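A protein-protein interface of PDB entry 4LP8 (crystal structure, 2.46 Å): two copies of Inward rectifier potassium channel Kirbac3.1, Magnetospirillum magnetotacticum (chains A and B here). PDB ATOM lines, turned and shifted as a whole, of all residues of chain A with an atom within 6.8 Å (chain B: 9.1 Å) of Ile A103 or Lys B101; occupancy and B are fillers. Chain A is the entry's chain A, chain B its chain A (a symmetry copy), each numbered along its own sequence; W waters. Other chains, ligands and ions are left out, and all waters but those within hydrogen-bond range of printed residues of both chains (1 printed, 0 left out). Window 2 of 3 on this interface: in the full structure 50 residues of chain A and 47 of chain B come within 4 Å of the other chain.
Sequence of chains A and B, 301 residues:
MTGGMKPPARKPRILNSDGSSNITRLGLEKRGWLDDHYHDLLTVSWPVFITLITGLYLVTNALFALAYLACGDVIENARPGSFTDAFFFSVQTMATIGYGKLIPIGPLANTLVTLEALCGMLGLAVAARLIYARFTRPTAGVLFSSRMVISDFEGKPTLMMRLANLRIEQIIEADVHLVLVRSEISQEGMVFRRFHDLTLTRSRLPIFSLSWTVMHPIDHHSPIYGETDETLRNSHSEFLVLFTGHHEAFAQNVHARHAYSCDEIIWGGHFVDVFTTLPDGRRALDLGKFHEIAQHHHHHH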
ATOM      1  N   VAL A  74       6.743  17.074   8.304  1.00  0.00           N
ATOM      2  CA  VAL A  74       5.980  16.954   7.065  1.00  0.00           C
ATOM      3  C   VAL A  74       4.571  16.357   7.283  1.00  0.00           C
ATOM      4  O   VAL A  74       3.938  15.938   6.311  1.00  0.00           O
ATOM      5  CB  VAL A  74       6.791  16.152   6.012  1.00  0.00           C
ATOM      6  CG1 VAL A  74       8.006  16.939   5.532  1.00  0.00           C
ATOM      7  CG2 VAL A  74       7.204  14.775   6.545  1.00  0.00           C
ATOM      8  N   ILE A  75       4.076  16.346   8.546  1.00  0.00           N
ATOM      9  CA  ILE A  75       2.745  15.851   8.928  1.00  0.00           C
ATOM     10  C   ILE A  75       2.007  17.002   9.659  1.00  0.00           C
ATOM     11  O   ILE A  75       2.427  17.388  10.750  1.00  0.00           O
ATOM     12  CB  ILE A  75       2.820  14.554   9.807  1.00  0.00           C
ATOM     13  CG1 ILE A  75       3.640  13.435   9.136  1.00  0.00           C
ATOM     14  CG2 ILE A  75       1.422  14.054  10.221  1.00  0.00           C
ATOM     15  CD1 ILE A  75       4.279  12.454  10.098  1.00  0.00           C
ATOM     16  N   GLU A  76       0.925  17.542   9.060  1.00  0.00           N
ATOM     17  CA  GLU A  76       0.122  18.584   9.682  1.00  0.00           C
ATOM     18  C   GLU A  76      -0.536  18.049  10.950  1.00  0.00           C
ATOM     19  O   GLU A  76      -0.873  16.864  11.004  1.00  0.00           O
ATOM     20  CB  GLU A  76      -0.950  19.077   8.707  1.00  0.00           C
ATOM     21  CG  GLU A  76      -1.236  20.566   8.796  1.00  0.00           C
ATOM     22  CD  GLU A  76      -2.057  21.075   7.632  1.00  0.00           C
ATOM     23  OE1 GLU A  76      -1.586  20.966   6.476  1.00  0.00           O
ATOM     24  OE2 GLU A  76      -3.190  21.549   7.873  1.00  0.00           O
ATOM     25  N   ASN A  77      -0.693  18.918  11.978  1.00  0.00           N
ATOM     26  CA  ASN A  77      -1.299  18.605  13.293  1.00  0.00           C
ATOM     27  C   ASN A  77      -0.532  17.508  14.087  1.00  0.00           C
ATOM     28  O   ASN A  77      -1.071  16.951  15.057  1.00  0.00           O
ATOM     29  CB  ASN A  77      -2.788  18.266  13.170  1.00  0.00           C
ATOM     30  CG  ASN A  77      -3.547  19.434  12.606  1.00  0.00           C
ATOM     31  OD1 ASN A  77      -3.913  20.355  13.329  1.00  0.00           O
ATOM     32  ND2 ASN A  77      -3.665  19.502  11.284  1.00  0.00           N
ATOM     33  N   ALA A  78       0.743  17.262  13.720  1.00  0.00           N
ATOM     34  CA  ALA A  78       1.627  16.370  14.449  1.00  0.00           C
ATOM     35  C   ALA A  78       2.644  17.191  15.237  1.00  0.00           C
ATOM     36  O   ALA A  78       3.125  18.236  14.761  1.00  0.00           O
ATOM     37  CB  ALA A  78       2.336  15.422  13.509  1.00  0.00           C
ATOM     38  N   PHE A  89      -0.071   8.385  12.069  1.00  0.00           N
ATOM     39  CA  PHE A  89      -0.321   8.872  10.710  1.00  0.00           C
ATOM     40  C   PHE A  89      -0.026   7.732   9.681  1.00  0.00           C
ATOM     41  O   PHE A  89      -0.852   7.474   8.797  1.00  0.00           O
ATOM     42  CB  PHE A  89       0.492  10.130  10.411  1.00  0.00           C
ATOM     43  CG  PHE A  89       0.512  10.486   8.950  1.00  0.00           C
ATOM     44  CD1 PHE A  89      -0.621  10.968   8.322  1.00  0.00           C
ATOM     45  CD2 PHE A  89       1.670  10.339   8.200  1.00  0.00           C
ATOM     46  CE1 PHE A  89      -0.602  11.295   6.966  1.00  0.00           C
ATOM     47  CE2 PHE A  89       1.684  10.663   6.842  1.00  0.00           C
ATOM     48  CZ  PHE A  89       0.553  11.160   6.240  1.00  0.00           C
ATOM     49  N   GLN A  92      -2.868   5.219   9.630  1.00  0.00           N
ATOM     50  CA  GLN A  92      -3.994   5.870   8.943  1.00  0.00           C
ATOM     51  C   GLN A  92      -3.798   5.897   7.421  1.00  0.00           C
ATOM     52  O   GLN A  92      -4.783   5.912   6.684  1.00  0.00           O
ATOM     53  CB  GLN A  92      -4.183   7.293   9.488  1.00  0.00           C
ATOM     54  CG  GLN A  92      -4.803   7.290  10.884  1.00  0.00           C
ATOM     55  CD  GLN A  92      -4.809   8.623  11.604  1.00  0.00           C
ATOM     56  OE1 GLN A  92      -4.829   9.734  11.018  1.00  0.00           O
ATOM     57  NE2 GLN A  92      -4.877   8.521  12.917  1.00  0.00           N
ATOM     58  N   GLY A  98      -7.423   7.366   6.755  1.00  0.00           N
ATOM     59  CA  GLY A  98      -7.283   8.763   6.386  1.00  0.00           C
ATOM     60  C   GLY A  98      -8.306   9.705   6.951  1.00  0.00           C
ATOM     61  O   GLY A  98      -8.995  10.386   6.194  1.00  0.00           O
ATOM     62  N   TYR A  99      -8.371   9.785   8.292  1.00  0.00           N
ATOM     63  CA  TYR A  99      -9.276  10.656   9.017  1.00  0.00           C
ATOM     64  C   TYR A  99      -9.154  12.073   8.493  1.00  0.00           C
ATOM     65  O   TYR A  99     -10.160  12.675   8.124  1.00  0.00           O
ATOM     66  CB  TYR A  99      -8.964  10.608  10.523  1.00  0.00           C
ATOM     67  CG  TYR A  99      -9.243   9.270  11.174  1.00  0.00           C
ATOM     68  CD1 TYR A  99     -10.542   8.766  11.255  1.00  0.00           C
ATOM     69  CD2 TYR A  99      -8.227   8.557  11.807  1.00  0.00           C
ATOM     70  CE1 TYR A  99     -10.810   7.553  11.875  1.00  0.00           C
ATOM     71  CE2 TYR A  99      -8.486   7.345  12.448  1.00  0.00           C
ATOM     72  CZ  TYR A  99      -9.781   6.847  12.484  1.00  0.00           C
ATOM     73  OH  TYR A  99     -10.060   5.672  13.148  1.00  0.00           O
ATOM     74  N   GLY A 100      -7.926  12.583   8.426  1.00  0.00           N
ATOM     75  CA  GLY A 100      -7.702  13.926   7.916  1.00  0.00           C
ATOM     76  C   GLY A 100      -7.237  14.984   8.899  1.00  0.00           C
ATOM     77  O   GLY A 100      -7.117  16.138   8.503  1.00  0.00           O
ATOM     78  N   LYS A 101      -6.941  14.605  10.166  1.00  0.00           N
ATOM     79  CA  LYS A 101      -6.329  15.482  11.160  1.00  0.00           C
ATOM     80  C   LYS A 101      -4.811  15.496  10.849  1.00  0.00           C
ATOM     81  O   LYS A 101      -4.235  16.558  10.644  1.00  0.00           O
ATOM     82  CB  LYS A 101      -6.656  15.016  12.606  1.00  0.00           C
ATOM     83  CG  LYS A 101      -5.944  15.773  13.739  1.00  0.00           C
ATOM     84  CD  LYS A 101      -6.652  17.053  14.171  1.00  0.00           C
ATOM     85  N   LEU A 102      -4.185  14.311  10.787  1.00  0.00           N
ATOM     86  CA  LEU A 102      -2.776  14.147  10.415  1.00  0.00           C
ATOM     87  C   LEU A 102      -2.750  13.955   8.899  1.00  0.00           C
ATOM     88  O   LEU A 102      -3.345  12.992   8.403  1.00  0.00           O
ATOM     89  CB  LEU A 102      -2.123  12.967  11.146  1.00  0.00           C
ATOM     90  CG  LEU A 102      -2.159  12.941  12.674  1.00  0.00           C
ATOM     91  CD1 LEU A 102      -1.780  11.556  13.175  1.00  0.00           C
ATOM     92  CD2 LEU A 102      -1.230  13.988  13.282  1.00  0.00           C
ATOM     93  N   ILE A 103      -2.201  14.937   8.162  1.00  0.00           N
ATOM     94  CA  ILE A 103      -2.202  14.947   6.696  1.00  0.00           C
ATOM     95  C   ILE A 103      -0.800  15.276   6.190  1.00  0.00           C
ATOM     96  O   ILE A 103      -0.075  15.975   6.899  1.00  0.00           O
ATOM     97  CB  ILE A 103      -3.303  15.868   6.078  1.00  0.00           C
ATOM     98  CG1 ILE A 103      -3.219  17.322   6.520  1.00  0.00           C
ATOM     99  CG2 ILE A 103      -4.680  15.314   6.338  1.00  0.00           C
ATOM    100  CD1 ILE A 103      -3.921  18.322   5.591  1.00  0.00           C
ATOM    101  N   PRO A 104      -0.376  14.770   5.004  1.00  0.00           N
ATOM    102  CA  PRO A 104       1.013  15.020   4.555  1.00  0.00           C
ATOM    103  C   PRO A 104       1.226  16.399   3.949  1.00  0.00           C
ATOM    104  O   PRO A 104       0.323  16.952   3.334  1.00  0.00           O
ATOM    105  CB  PRO A 104       1.250  13.913   3.505  1.00  0.00           C
ATOM    106  CG  PRO A 104      -0.103  13.645   2.928  1.00  0.00           C
ATOM    107  CD  PRO A 104      -1.104  13.899   4.044  1.00  0.00           C
ATOM    108  N   ILE A 105       2.439  16.941   4.113  1.00  0.00           N
ATOM    109  CA  ILE A 105       2.855  18.248   3.586  1.00  0.00           C
ATOM    110  C   ILE A 105       4.090  18.070   2.701  1.00  0.00           C
ATOM    111  O   ILE A 105       5.063  17.440   3.114  1.00  0.00           O
ATOM    112  CB  ILE A 105       3.142  19.270   4.728  1.00  0.00           C
ATOM    113  CG1 ILE A 105       1.926  19.516   5.606  1.00  0.00           C
ATOM    114  CG2 ILE A 105       3.685  20.614   4.187  1.00  0.00           C
ATOM    115  CD1 ILE A 105       2.312  19.985   6.993  1.00  0.00           C
ATOM    116  N   ALA A 109       6.616  13.800   1.801  1.00  0.00           N
ATOM    117  CA  ALA A 109       5.656  13.012   2.556  1.00  0.00           C
ATOM    118  C   ALA A 109       4.580  12.453   1.659  1.00  0.00           C
ATOM    119  O   ALA A 109       4.073  11.366   1.937  1.00  0.00           O
ATOM    120  CB  ALA A 109       5.028  13.854   3.652  1.00  0.00           C
ATOM    121  N   VAL A 113       3.554   8.572   1.177  1.00  0.00           N
ATOM    122  CA  VAL A 113       2.139   8.186   1.331  1.00  0.00           C
ATOM    123  C   VAL A 113       1.772   7.257   0.143  1.00  0.00           C
ATOM    124  O   VAL A 113       1.166   6.197   0.334  1.00  0.00           O
ATOM    125  CB  VAL A 113       1.240   9.469   1.425  1.00  0.00           C
ATOM    126  CG1 VAL A 113      -0.212   9.206   1.009  1.00  0.00           C
ATOM    127  CG2 VAL A 113       1.293  10.079   2.819  1.00  0.00           C
ATOM    128  N   ILE B  75     -10.407  20.351  -8.076  1.00  0.00           N
ATOM    129  CA  ILE B  75      -9.867  19.778  -6.834  1.00  0.00           C
ATOM    130  C   ILE B  75      -9.702  20.936  -5.815  1.00  0.00           C
ATOM    131  O   ILE B  75      -8.872  21.818  -6.038  1.00  0.00           O
ATOM    132  CB  ILE B  75      -8.520  19.009  -7.067  1.00  0.00           C
ATOM    133  CG1 ILE B  75      -8.644  17.922  -8.153  1.00  0.00           C
ATOM    134  CG2 ILE B  75      -7.950  18.431  -5.757  1.00  0.00           C
ATOM    135  CD1 ILE B  75      -7.348  17.591  -8.867  1.00  0.00           C
ATOM    136  N   GLU B  76     -10.486  20.930  -4.717  1.00  0.00           N
ATOM    137  CA  GLU B  76     -10.373  21.932  -3.668  1.00  0.00           C
ATOM    138  C   GLU B  76      -9.006  21.836  -2.998  1.00  0.00           C
ATOM    139  O   GLU B  76      -8.459  20.736  -2.894  1.00  0.00           O
ATOM    140  CB  GLU B  76     -11.478  21.733  -2.627  1.00  0.00           C
ATOM    141  CG  GLU B  76     -12.033  23.023  -2.051  1.00  0.00           C
ATOM    142  CD  GLU B  76     -13.311  22.815  -1.272  1.00  0.00           C
ATOM    143  OE1 GLU B  76     -14.307  22.347  -1.872  1.00  0.00           O
ATOM    144  OE2 GLU B  76     -13.309  23.086  -0.050  1.00  0.00           O
ATOM    145  N   ASN B  77      -8.446  22.993  -2.571  1.00  0.00           N
ATOM    146  CA  ASN B  77      -7.129  23.124  -1.904  1.00  0.00           C
ATOM    147  C   ASN B  77      -5.936  22.648  -2.783  1.00  0.00           C
ATOM    148  O   ASN B  77      -4.828  22.437  -2.264  1.00  0.00           O
ATOM    149  CB  ASN B  77      -7.114  22.448  -0.530  1.00  0.00           C
ATOM    150  CG  ASN B  77      -8.130  23.083   0.378  1.00  0.00           C
ATOM    151  OD1 ASN B  77      -7.869  24.115   0.989  1.00  0.00           O
ATOM    152  ND2 ASN B  77      -9.357  22.574   0.370  1.00  0.00           N
ATOM    153  N   ALA B  78      -6.149  22.559  -4.112  1.00  0.00           N
ATOM    154  CA  ALA B  78      -5.100  22.264  -5.072  1.00  0.00           C
ATOM    155  C   ALA B  78      -4.723  23.537  -5.824  1.00  0.00           C
ATOM    156  O   ALA B  78      -5.591  24.371  -6.141  1.00  0.00           O
ATOM    157  CB  ALA B  78      -5.541  21.194  -6.044  1.00  0.00           C
ATOM    158  N   ASP B  85      -0.388  18.180  -7.301  1.00  0.00           N
ATOM    159  CA  ASP B  85      -1.591  18.215  -6.482  1.00  0.00           C
ATOM    160  C   ASP B  85      -2.658  17.259  -7.047  1.00  0.00           C
ATOM    161  O   ASP B  85      -3.267  16.513  -6.278  1.00  0.00           O
ATOM    162  CB  ASP B  85      -2.134  19.664  -6.369  1.00  0.00           C
ATOM    163  CG  ASP B  85      -1.329  20.634  -5.507  1.00  0.00           C
ATOM    164  OD1 ASP B  85      -0.162  20.330  -5.193  1.00  0.00           O
ATOM    165  OD2 ASP B  85      -1.852  21.710  -5.182  1.00  0.00           O
ATOM    166  N   PHE B  89      -3.891  13.848  -5.206  1.00  0.00           N
ATOM    167  CA  PHE B  89      -5.330  13.665  -5.009  1.00  0.00           C
ATOM    168  C   PHE B  89      -5.775  12.298  -5.624  1.00  0.00           C
ATOM    169  O   PHE B  89      -6.476  11.525  -4.959  1.00  0.00           O
ATOM    170  CB  PHE B  89      -6.125  14.833  -5.590  1.00  0.00           C
ATOM    171  CG  PHE B  89      -7.599  14.552  -5.692  1.00  0.00           C
ATOM    172  CD1 PHE B  89      -8.385  14.472  -4.557  1.00  0.00           C
ATOM    173  CD2 PHE B  89      -8.202  14.366  -6.927  1.00  0.00           C
ATOM    174  CE1 PHE B  89      -9.751  14.207  -4.653  1.00  0.00           C
ATOM    175  CE2 PHE B  89      -9.569  14.098  -7.019  1.00  0.00           C
ATOM    176  CZ  PHE B  89     -10.338  14.042  -5.881  1.00  0.00           C
ATOM    177  N   GLN B  92      -4.790   9.430  -3.343  1.00  0.00           N
ATOM    178  CA  GLN B  92      -5.701   9.477  -2.189  1.00  0.00           C
ATOM    179  C   GLN B  92      -7.088   8.918  -2.532  1.00  0.00           C
ATOM    180  O   GLN B  92      -7.774   8.412  -1.645  1.00  0.00           O
ATOM    181  CB  GLN B  92      -5.813  10.919  -1.673  1.00  0.00           C
ATOM    182  CG  GLN B  92      -4.555  11.355  -0.924  1.00  0.00           C
ATOM    183  CD  GLN B  92      -4.468  12.830  -0.586  1.00  0.00           C
ATOM    184  OE1 GLN B  92      -5.471  13.567  -0.412  1.00  0.00           O
ATOM    185  NE2 GLN B  92      -3.237  13.264  -0.403  1.00  0.00           N
ATOM    186  N   ILE B  97      -7.739   6.426   0.453  1.00  0.00           N
ATOM    187  CA  ILE B  97      -7.276   7.031   1.715  1.00  0.00           C
ATOM    188  C   ILE B  97      -8.252   8.151   2.094  1.00  0.00           C
ATOM    189  O   ILE B  97      -8.865   8.089   3.151  1.00  0.00           O
ATOM    190  CB  ILE B  97      -5.806   7.551   1.687  1.00  0.00           C
ATOM    191  CG1 ILE B  97      -4.808   6.452   1.274  1.00  0.00           C
ATOM    192  CG2 ILE B  97      -5.444   8.124   3.073  1.00  0.00           C
ATOM    193  CD1 ILE B  97      -3.496   6.972   0.712  1.00  0.00           C
ATOM    194  N   GLY B  98      -8.358   9.150   1.220  1.00  0.00           N
ATOM    195  CA  GLY B  98      -9.283  10.265   1.315  1.00  0.00           C
ATOM    196  C   GLY B  98      -9.182  11.106   2.555  1.00  0.00           C
ATOM    197  O   GLY B  98     -10.164  11.246   3.280  1.00  0.00           O
ATOM    198  N   TYR B  99      -8.002  11.714   2.771  1.00  0.00           N
ATOM    199  CA  TYR B  99      -7.726  12.585   3.898  1.00  0.00           C
ATOM    200  C   TYR B  99      -8.800  13.650   3.999  1.00  0.00           C
ATOM    201  O   TYR B  99      -9.401  13.811   5.059  1.00  0.00           O
ATOM    202  CB  TYR B  99      -6.338  13.230   3.740  1.00  0.00           C
ATOM    203  CG  TYR B  99      -5.185  12.253   3.820  1.00  0.00           C
ATOM    204  CD1 TYR B  99      -4.913  11.556   4.999  1.00  0.00           C
ATOM    205  CD2 TYR B  99      -4.297  12.106   2.757  1.00  0.00           C
ATOM    206  CE1 TYR B  99      -3.840  10.680   5.090  1.00  0.00           C
ATOM    207  CE2 TYR B  99      -3.205  11.240   2.841  1.00  0.00           C
ATOM    208  CZ  TYR B  99      -2.978  10.530   4.012  1.00  0.00           C
ATOM    209  OH  TYR B  99      -1.881   9.703   4.125  1.00  0.00           O
ATOM    210  N   GLY B 100      -9.062  14.343   2.893  1.00  0.00           N
ATOM    211  CA  GLY B 100     -10.091  15.371   2.882  1.00  0.00           C
ATOM    212  C   GLY B 100      -9.643  16.812   2.734  1.00  0.00           C
ATOM    213  O   GLY B 100     -10.490  17.697   2.799  1.00  0.00           O
ATOM    214  N   LYS B 101      -8.332  17.063   2.503  1.00  0.00           N
ATOM    215  CA  LYS B 101      -7.796  18.382   2.179  1.00  0.00           C
ATOM    216  C   LYS B 101      -8.066  18.599   0.668  1.00  0.00           C
ATOM    217  O   LYS B 101      -8.695  19.581   0.291  1.00  0.00           O
ATOM    218  CB  LYS B 101      -6.294  18.493   2.557  1.00  0.00           C
ATOM    219  CG  LYS B 101      -5.580  19.785   2.126  1.00  0.00           C
ATOM    220  CD  LYS B 101      -5.739  20.940   3.109  1.00  0.00           C
ATOM    221  N   LEU B 102      -7.613  17.662  -0.178  1.00  0.00           N
ATOM    222  CA  LEU B 102      -7.863  17.673  -1.624  1.00  0.00           C
ATOM    223  C   LEU B 102      -9.155  16.885  -1.843  1.00  0.00           C
ATOM    224  O   LEU B 102      -9.201  15.699  -1.500  1.00  0.00           O
ATOM    225  CB  LEU B 102      -6.693  17.073  -2.413  1.00  0.00           C
ATOM    226  CG  LEU B 102      -5.299  17.670  -2.225  1.00  0.00           C
ATOM    227  CD1 LEU B 102      -4.253  16.735  -2.811  1.00  0.00           C
ATOM    228  CD2 LEU B 102      -5.181  19.050  -2.866  1.00  0.00           C
ATOM    229  N   ILE B 103     -10.231  17.572  -2.265  1.00  0.00           N
ATOM    230  CA  ILE B 103     -11.563  16.977  -2.413  1.00  0.00           C
ATOM    231  C   ILE B 103     -12.144  17.367  -3.769  1.00  0.00           C
ATOM    232  O   ILE B 103     -11.790  18.435  -4.269  1.00  0.00           O
ATOM    233  CB  ILE B 103     -12.527  17.296  -1.225  1.00  0.00           C
ATOM    234  CG1 ILE B 103     -12.742  18.783  -0.979  1.00  0.00           C
ATOM    235  CG2 ILE B 103     -12.073  16.611   0.039  1.00  0.00           C
ATOM    236  CD1 ILE B 103     -14.015  19.131  -0.197  1.00  0.00           C
ATOM    237  N   PRO B 104     -12.999  16.524  -4.404  1.00  0.00           N
ATOM    238  CA  PRO B 104     -13.495  16.865  -5.757  1.00  0.00           C
ATOM    239  C   PRO B 104     -14.626  17.882  -5.761  1.00  0.00           C
ATOM    240  O   PRO B 104     -15.428  17.921  -4.836  1.00  0.00           O
ATOM    241  CB  PRO B 104     -13.974  15.505  -6.311  1.00  0.00           C
ATOM    242  CG  PRO B 104     -14.398  14.735  -5.103  1.00  0.00           C
ATOM    243  CD  PRO B 104     -13.507  15.199  -3.961  1.00  0.00           C
ATOM    244  N   ILE B 105     -14.693  18.695  -6.822  1.00  0.00           N
ATOM    245  CA  ILE B 105     -15.719  19.726  -7.030  1.00  0.00           C
ATOM    246  C   ILE B 105     -16.430  19.475  -8.361  1.00  0.00           C
ATOM    247  O   ILE B 105     -15.777  19.301  -9.389  1.00  0.00           O
ATOM    248  CB  ILE B 105     -15.115  21.162  -6.994  1.00  0.00           C
ATOM    249  CG1 ILE B 105     -14.438  21.476  -5.669  1.00  0.00           C
ATOM    250  CG2 ILE B 105     -16.168  22.249  -7.319  1.00  0.00           C
ATOM    251  CD1 ILE B 105     -13.377  22.545  -5.811  1.00  0.00           C
HETATM  252  O   HOH W   1      -8.714  16.411   6.058  1.00  0.00           O
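Water W1 bridges the backbone carbonyl oxygen of Tyr B99 (2.9 Å) and the backbone carbonyl oxygen of Gly A100 (2.9 Å).
Tyr B99 touches Phe A89.
Gly A98 touches Ile B97.
Gly A98 touches Tyr B99 (O to CA, 3.4 Å).
Gly A100 touches Tyr B99 (CA to O, 3.3 Å).
Ile A103 touches Tyr B99 (CG2 to CB, 3.7 Å).
Lys B101 touches Ile A103 (CB to CD1, 3.9 Å).
Pro A104 touches Tyr B99 (CD to CE2, 3.6 Å).
Val A113 touches Ile B97.
Tyr B99 touches Val A113 (OH to CG2, 3.5 Å).
The backbone carbonyl oxygen (O) of Lys B101 lies within hydrogen-bond range of the side-chain amide nitrogen (ND2) of Asn B77, 3.1 Å away.
O of Gln B92 sits at hydrogen-bond distance from N of Gly B98 (3.0 Å).
The backbone carbonyl oxygen (O) of Gln A92 is in hydrogen-bond range of the backbone NH (N) of Gly A98 (3.0 Å).
N of Glu A76 lies within hydrogen-bond range of O of Ile A103 (2.9 Å).
The backbone carbonyl oxygen (O) of Gln B92 lies within hydrogen-bond range of the backbone NH (N) of Ile B97 (2.9 Å).
Of the 17 printed residues of chain A, 7 touch a printed residue of chain B.
Hydrophobic or aromatic side chains of chain A within 4 Å of the printed part of chain B: Phe A89, Ile A103, Pro A104 and Val A113.
Of the 16 printed residues of chain B, 4 touch a printed residue of chain A.
Printed residues of chain B that touch a printed residue of chain A: Ile B97, Gly B98, Tyr B99 and Lys B101.
Hydrophobic or aromatic side chains of chain B that line the printed part of chain A: Ile B97 and Tyr B99.
Among the printed residues, 11 pairs touch across the chains.
Among the printed residues, no Asp or Glu carboxylate lies within 4 Å of a Lys or Arg side-chain nitrogen of the other chain.
Phe A89 touches Tyr B99, but with the chains exchanged Tyr A99 does not touch Phe B89 (12.9 Å).
Tyr A99 touches its own counterpart, Tyr B99.
Ile A103 touches Tyr B99, but with the chains exchanged Tyr A99 does not touch Ile B103 (9.2 Å).
Ile A103 touches Lys B101, but with the chains exchanged Lys A101 does not touch Ile B103 (11.5 Å).
Positions printed for both chains: 75, 76, 77, 78, 89, 92, 98, 99, 100, 101, 102, 103, 104 and 105.
The backbone carbonyl oxygen (O) of Gly A98 sits close to the backbone carbonyl oxygen (O) of Gly B98, 3.3 Å away.
The backbone carbonyl oxygen of Tyr B99 sits close to the backbone carbonyl oxygen of Tyr A99.
No residue of chain B comes within 4 Å of Glu A76.
Of chain B, only Tyr B99 comes within 4 Å of Gly A100.
Ile A103 touches two residues of chain B.
Pro A104 touches just one residue of chain B: Tyr B99 (3.6 Å).
Printed residues of chain B within 4 Å of Val A113: Ile B97 and Tyr B99.
Asp B85 touches none of the printed residues of chain A.
Of the printed residues of chain A, Gly B98 touches Gly A98.
Printed residues of chain A within 4 Å of Tyr B99: Phe A89, Gly A98, Tyr A99, Gly A100, Ile A103, Pro A104 and Val A113.
Gly B100 touches none of the printed residues of chain A.
Of the printed residues of chain A, Lys B101 touches Ile A103 (3.9 Å).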
